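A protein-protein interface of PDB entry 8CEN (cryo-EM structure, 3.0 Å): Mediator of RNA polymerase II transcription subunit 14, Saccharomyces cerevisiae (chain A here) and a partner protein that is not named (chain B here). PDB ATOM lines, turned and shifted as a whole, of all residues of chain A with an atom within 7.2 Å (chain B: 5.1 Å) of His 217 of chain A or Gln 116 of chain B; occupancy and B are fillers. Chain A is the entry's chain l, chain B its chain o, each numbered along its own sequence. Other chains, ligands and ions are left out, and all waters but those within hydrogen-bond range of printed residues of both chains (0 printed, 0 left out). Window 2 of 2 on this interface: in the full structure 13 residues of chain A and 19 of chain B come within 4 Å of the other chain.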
ATOM      1  N   LEU A 214     -28.605 -18.933   4.050  1.00  0.00           N
ATOM      2  CA  LEU A 214     -28.143 -19.799   5.121  1.00  0.00           C
ATOM      3  C   LEU A 214     -28.705 -21.197   4.908  1.00  0.00           C
ATOM      4  O   LEU A 214     -29.708 -21.367   4.204  1.00  0.00           O
ATOM      5  CB  LEU A 214     -28.578 -19.268   6.496  1.00  0.00           C
ATOM      6  CG  LEU A 214     -27.817 -18.097   7.116  1.00  0.00           C
ATOM      7  CD1 LEU A 214     -28.360 -16.778   6.621  1.00  0.00           C
ATOM      8  CD2 LEU A 214     -27.871 -18.162   8.636  1.00  0.00           C
ATOM      9  N   PRO A 215     -28.059 -22.228   5.459  1.00  0.00           N
ATOM     10  CA  PRO A 215     -28.621 -23.583   5.365  1.00  0.00           C
ATOM     11  C   PRO A 215     -29.972 -23.680   6.060  1.00  0.00           C
ATOM     12  O   PRO A 215     -30.155 -23.194   7.177  1.00  0.00           O
ATOM     13  CB  PRO A 215     -27.566 -24.452   6.058  1.00  0.00           C
ATOM     14  CG  PRO A 215     -26.300 -23.694   5.914  1.00  0.00           C
ATOM     15  CD  PRO A 215     -26.674 -22.243   5.964  1.00  0.00           C
ATOM     16  N   THR A 216     -30.923 -24.317   5.380  1.00  0.00           N
ATOM     17  CA  THR A 216     -32.283 -24.481   5.875  1.00  0.00           C
ATOM     18  C   THR A 216     -32.562 -25.965   6.052  1.00  0.00           C
ATOM     19  O   THR A 216     -32.411 -26.747   5.107  1.00  0.00           O
ATOM     20  CB  THR A 216     -33.302 -23.861   4.916  1.00  0.00           C
ATOM     21  OG1 THR A 216     -33.312 -24.598   3.687  1.00  0.00           O
ATOM     22  CG2 THR A 216     -32.951 -22.411   4.626  1.00  0.00           C
ATOM     23  N   HIS A 217     -32.964 -26.352   7.261  1.00  0.00           N
ATOM     24  CA  HIS A 217     -33.325 -27.733   7.546  1.00  0.00           C
ATOM     25  C   HIS A 217     -34.826 -27.939   7.681  1.00  0.00           C
ATOM     26  O   HIS A 217     -35.299 -29.068   7.511  1.00  0.00           O
ATOM     27  CB  HIS A 217     -32.630 -28.203   8.827  1.00  0.00           C
ATOM     28  CG  HIS A 217     -31.223 -27.710   8.959  1.00  0.00           C
ATOM     29  ND1 HIS A 217     -30.870 -26.690   9.816  1.00  0.00           N
ATOM     30  CD2 HIS A 217     -30.083 -28.086   8.332  1.00  0.00           C
ATOM     31  CE1 HIS A 217     -29.573 -26.462   9.716  1.00  0.00           C
ATOM     32  NE2 HIS A 217     -29.071 -27.297   8.823  1.00  0.00           N
ATOM     33  N   ASN A 218     -35.575 -26.882   7.975  1.00  0.00           N
ATOM     34  CA  ASN A 218     -37.023 -26.925   8.092  1.00  0.00           C
ATOM     35  C   ASN A 218     -37.656 -26.126   6.960  1.00  0.00           C
ATOM     36  O   ASN A 218     -36.979 -25.420   6.210  1.00  0.00           O
ATOM     37  CB  ASN A 218     -37.475 -26.382   9.453  1.00  0.00           C
ATOM     38  CG  ASN A 218     -36.744 -27.036  10.611  1.00  0.00           C
ATOM     39  OD1 ASN A 218     -35.561 -26.786  10.835  1.00  0.00           O
ATOM     40  ND2 ASN A 218     -37.450 -27.882  11.351  1.00  0.00           N
ATOM     41  N   PHE A 219     -38.975 -26.254   6.838  1.00  0.00           N
ATOM     42  CA  PHE A 219     -39.696 -25.541   5.794  1.00  0.00           C
ATOM     43  C   PHE A 219     -39.767 -24.053   6.118  1.00  0.00           C
ATOM     44  O   PHE A 219     -39.880 -23.649   7.280  1.00  0.00           O
ATOM     45  CB  PHE A 219     -41.103 -26.109   5.626  1.00  0.00           C
ATOM     46  CG  PHE A 219     -41.907 -25.425   4.556  1.00  0.00           C
ATOM     47  CD1 PHE A 219     -41.510 -25.494   3.230  1.00  0.00           C
ATOM     48  CD2 PHE A 219     -43.046 -24.707   4.875  1.00  0.00           C
ATOM     49  CE1 PHE A 219     -42.239 -24.863   2.239  1.00  0.00           C
ATOM     50  CE2 PHE A 219     -43.781 -24.075   3.887  1.00  0.00           C
ATOM     51  CZ  PHE A 219     -43.376 -24.153   2.569  1.00  0.00           C
ATOM     52  N   GLN B 113     -31.389 -26.936  17.837  1.00  0.00           N
ATOM     53  CA  GLN B 113     -30.617 -26.458  16.698  1.00  0.00           C
ATOM     54  C   GLN B 113     -30.158 -25.010  16.842  1.00  0.00           C
ATOM     55  O   GLN B 113     -29.702 -24.420  15.859  1.00  0.00           O
ATOM     56  CB  GLN B 113     -31.434 -26.631  15.416  1.00  0.00           C
ATOM     57  CG  GLN B 113     -31.710 -28.089  15.073  1.00  0.00           C
ATOM     58  CD  GLN B 113     -32.528 -28.260  13.810  1.00  0.00           C
ATOM     59  OE1 GLN B 113     -32.955 -27.285  13.196  1.00  0.00           O
ATOM     60  NE2 GLN B 113     -32.754 -29.507  13.418  1.00  0.00           N
ATOM     61  N   GLY B 114     -30.266 -24.425  18.034  1.00  0.00           N
ATOM     62  CA  GLY B 114     -29.735 -23.109  18.296  1.00  0.00           C
ATOM     63  C   GLY B 114     -28.231 -22.985  18.151  1.00  0.00           C
ATOM     64  O   GLY B 114     -27.739 -22.148  17.384  1.00  0.00           O
ATOM     65  N   PRO B 115     -27.467 -23.787  18.912  1.00  0.00           N
ATOM     66  CA  PRO B 115     -26.004 -23.775  18.735  1.00  0.00           C
ATOM     67  C   PRO B 115     -25.554 -24.068  17.315  1.00  0.00           C
ATOM     68  O   PRO B 115     -24.613 -23.430  16.828  1.00  0.00           O
ATOM     69  CB  PRO B 115     -25.536 -24.855  19.717  1.00  0.00           C
ATOM     70  CG  PRO B 115     -26.538 -24.805  20.803  1.00  0.00           C
ATOM     71  CD  PRO B 115     -27.854 -24.513  20.137  1.00  0.00           C
ATOM     72  N   GLN B 116     -26.241 -24.975  16.621  1.00  0.00           N
ATOM     73  CA  GLN B 116     -25.891 -25.291  15.241  1.00  0.00           C
ATOM     74  C   GLN B 116     -26.154 -24.106  14.314  1.00  0.00           C
ATOM     75  O   GLN B 116     -25.322 -23.785  13.458  1.00  0.00           O
ATOM     76  CB  GLN B 116     -26.669 -26.526  14.789  1.00  0.00           C
ATOM     77  CG  GLN B 116     -26.045 -27.271  13.627  1.00  0.00           C
ATOM     78  CD  GLN B 116     -26.823 -27.100  12.346  1.00  0.00           C
ATOM     79  OE1 GLN B 116     -27.976 -26.670  12.360  1.00  0.00           O
ATOM     80  NE2 GLN B 116     -26.203 -27.449  11.226  1.00  0.00           N
ATOM     81  N   TRP B 117     -27.303 -23.440  14.477  1.00  0.00           N
ATOM     82  CA  TRP B 117     -27.629 -22.287  13.638  1.00  0.00           C
ATOM     83  C   TRP B 117     -26.668 -21.128  13.870  1.00  0.00           C
ATOM     84  O   TRP B 117     -26.218 -20.482  12.910  1.00  0.00           O
ATOM     85  CB  TRP B 117     -29.067 -21.839  13.895  1.00  0.00           C
ATOM     86  CG  TRP B 117     -30.086 -22.700  13.238  1.00  0.00           C
ATOM     87  CD1 TRP B 117     -29.899 -23.510  12.160  1.00  0.00           C
ATOM     88  CD2 TRP B 117     -31.451 -22.865  13.634  1.00  0.00           C
ATOM     89  NE1 TRP B 117     -31.068 -24.159  11.847  1.00  0.00           N
ATOM     90  CE2 TRP B 117     -32.036 -23.782  12.740  1.00  0.00           C
ATOM     91  CE3 TRP B 117     -32.236 -22.324  14.656  1.00  0.00           C
ATOM     92  CZ2 TRP B 117     -33.369 -24.167  12.834  1.00  0.00           C
ATOM     93  CZ3 TRP B 117     -33.558 -22.709  14.749  1.00  0.00           C
ATOM     94  CH2 TRP B 117     -34.111 -23.625  13.846  1.00  0.00           C
ATOM     95  N   MET B 118     -26.334 -20.846  15.133  1.00  0.00           N
ATOM     96  CA  MET B 118     -25.412 -19.742  15.369  1.00  0.00           C
ATOM     97  C   MET B 118     -23.996 -20.103  14.944  1.00  0.00           C
ATOM     98  O   MET B 118     -23.250 -19.227  14.496  1.00  0.00           O
ATOM     99  CB  MET B 118     -25.452 -19.283  16.827  1.00  0.00           C
ATOM    100  CG  MET B 118     -25.103 -20.314  17.862  1.00  0.00           C
ATOM    101  SD  MET B 118     -25.636 -19.733  19.479  1.00  0.00           S
ATOM    102  CE  MET B 118     -24.820 -18.141  19.526  1.00  0.00           C
ATOM    103  N   ASN B 119     -23.627 -21.387  15.016  1.00  0.00           N
ATOM    104  CA  ASN B 119     -22.341 -21.813  14.476  1.00  0.00           C
ATOM    105  C   ASN B 119     -22.290 -21.634  12.963  1.00  0.00           C
ATOM    106  O   ASN B 119     -21.279 -21.174  12.423  1.00  0.00           O
ATOM    107  CB  ASN B 119     -22.073 -23.267  14.859  1.00  0.00           C
ATOM    108  CG  ASN B 119     -21.254 -23.394  16.129  1.00  0.00           C
ATOM    109  OD1 ASN B 119     -20.935 -22.398  16.776  1.00  0.00           O
ATOM    110  ND2 ASN B 119     -20.907 -24.624  16.491  1.00  0.00           N
ATOM    111  N   GLU B 120     -23.379 -21.976  12.264  1.00  0.00           N
ATOM    112  CA  GLU B 120     -23.415 -21.801  10.812  1.00  0.00           C
ATOM    113  C   GLU B 120     -23.347 -20.331  10.417  1.00  0.00           C
ATOM    114  O   GLU B 120     -22.661 -19.976   9.451  1.00  0.00           O
ATOM    115  CB  GLU B 120     -24.667 -22.447  10.220  1.00  0.00           C
ATOM    116  CG  GLU B 120     -24.706 -23.963  10.297  1.00  0.00           C
ATOM    117  CD  GLU B 120     -25.982 -24.530   9.710  1.00  0.00           C
ATOM    118  OE1 GLU B 120     -26.880 -23.735   9.365  1.00  0.00           O
ATOM    119  OE2 GLU B 120     -26.082 -25.767   9.574  1.00  0.00           O
ATOM    120  N   MET B 121     -24.044 -19.453  11.144  1.00  0.00           N
ATOM    121  CA  MET B 121     -23.958 -18.041  10.784  1.00  0.00           C
ATOM    122  C   MET B 121     -22.629 -17.411  11.199  1.00  0.00           C
ATOM    123  O   MET B 121     -22.184 -16.460  10.550  1.00  0.00           O
ATOM    124  CB  MET B 121     -25.145 -17.260  11.358  1.00  0.00           C
ATOM    125  CG  MET B 121     -25.228 -17.191  12.858  1.00  0.00           C
ATOM    126  SD  MET B 121     -26.719 -16.344  13.428  1.00  0.00           S
ATOM    127  CE  MET B 121     -27.979 -17.565  13.080  1.00  0.00           C
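ND1 of His 217 of chain A is in hydrogen-bond range of NE1 of Trp 117 of chain B (3.3 Å). A ring nitrogen (NE2) of His 217 of chain A lies within hydrogen-bond range of the side-chain carboxylate of Glu 120 of chain B (3.4 Å).
OE1 of Gln 116 of chain B sits close to OE2 of Glu 120 of chain B (3.5 Å).
Among the printed residues, merely in contact across the chains: Leu 214 of chain A with Met 121 of chain B, Pro 215 of chain A with Glu 120 of chain B, His 217 of chain A with Gln 116 of chain B, Asn 218 of chain A with Gln 113 of chain B and Asn 218 of chain A with Trp 117 of chain B.
Of the printed residues of chain B, Leu 214 of chain A touches Met 121. Printed residues of chain B within 4 Å of Pro 215 of chain A: Glu 120 (3.5 Å). Of the printed residues of chain A, Gln 113 of chain B touches Asn 218. Of the printed residues of chain A, Gln 116 of chain B touches His 217 (3.1 Å). Met 118 of chain B touches none of the printed residues of chain A. Printed residues of chain A within 4 Å of Glu 120 of chain B: Pro 215 (3.5 Å) and His 217 (3.4 Å). Of the printed residues of chain A, Met 121 of chain B touches Leu 214.
Of the 6 printed residues of chain A, 4 touch a printed residue of chain B. Hydrophobic or aromatic side chains of chain A within 4 Å of the printed part of chain B: Leu 214, Pro 215 and His 217. Among the printed residues, no Asp or Glu carboxylate lies within 4 Å of a Lys or Arg side-chain nitrogen of the other chain.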
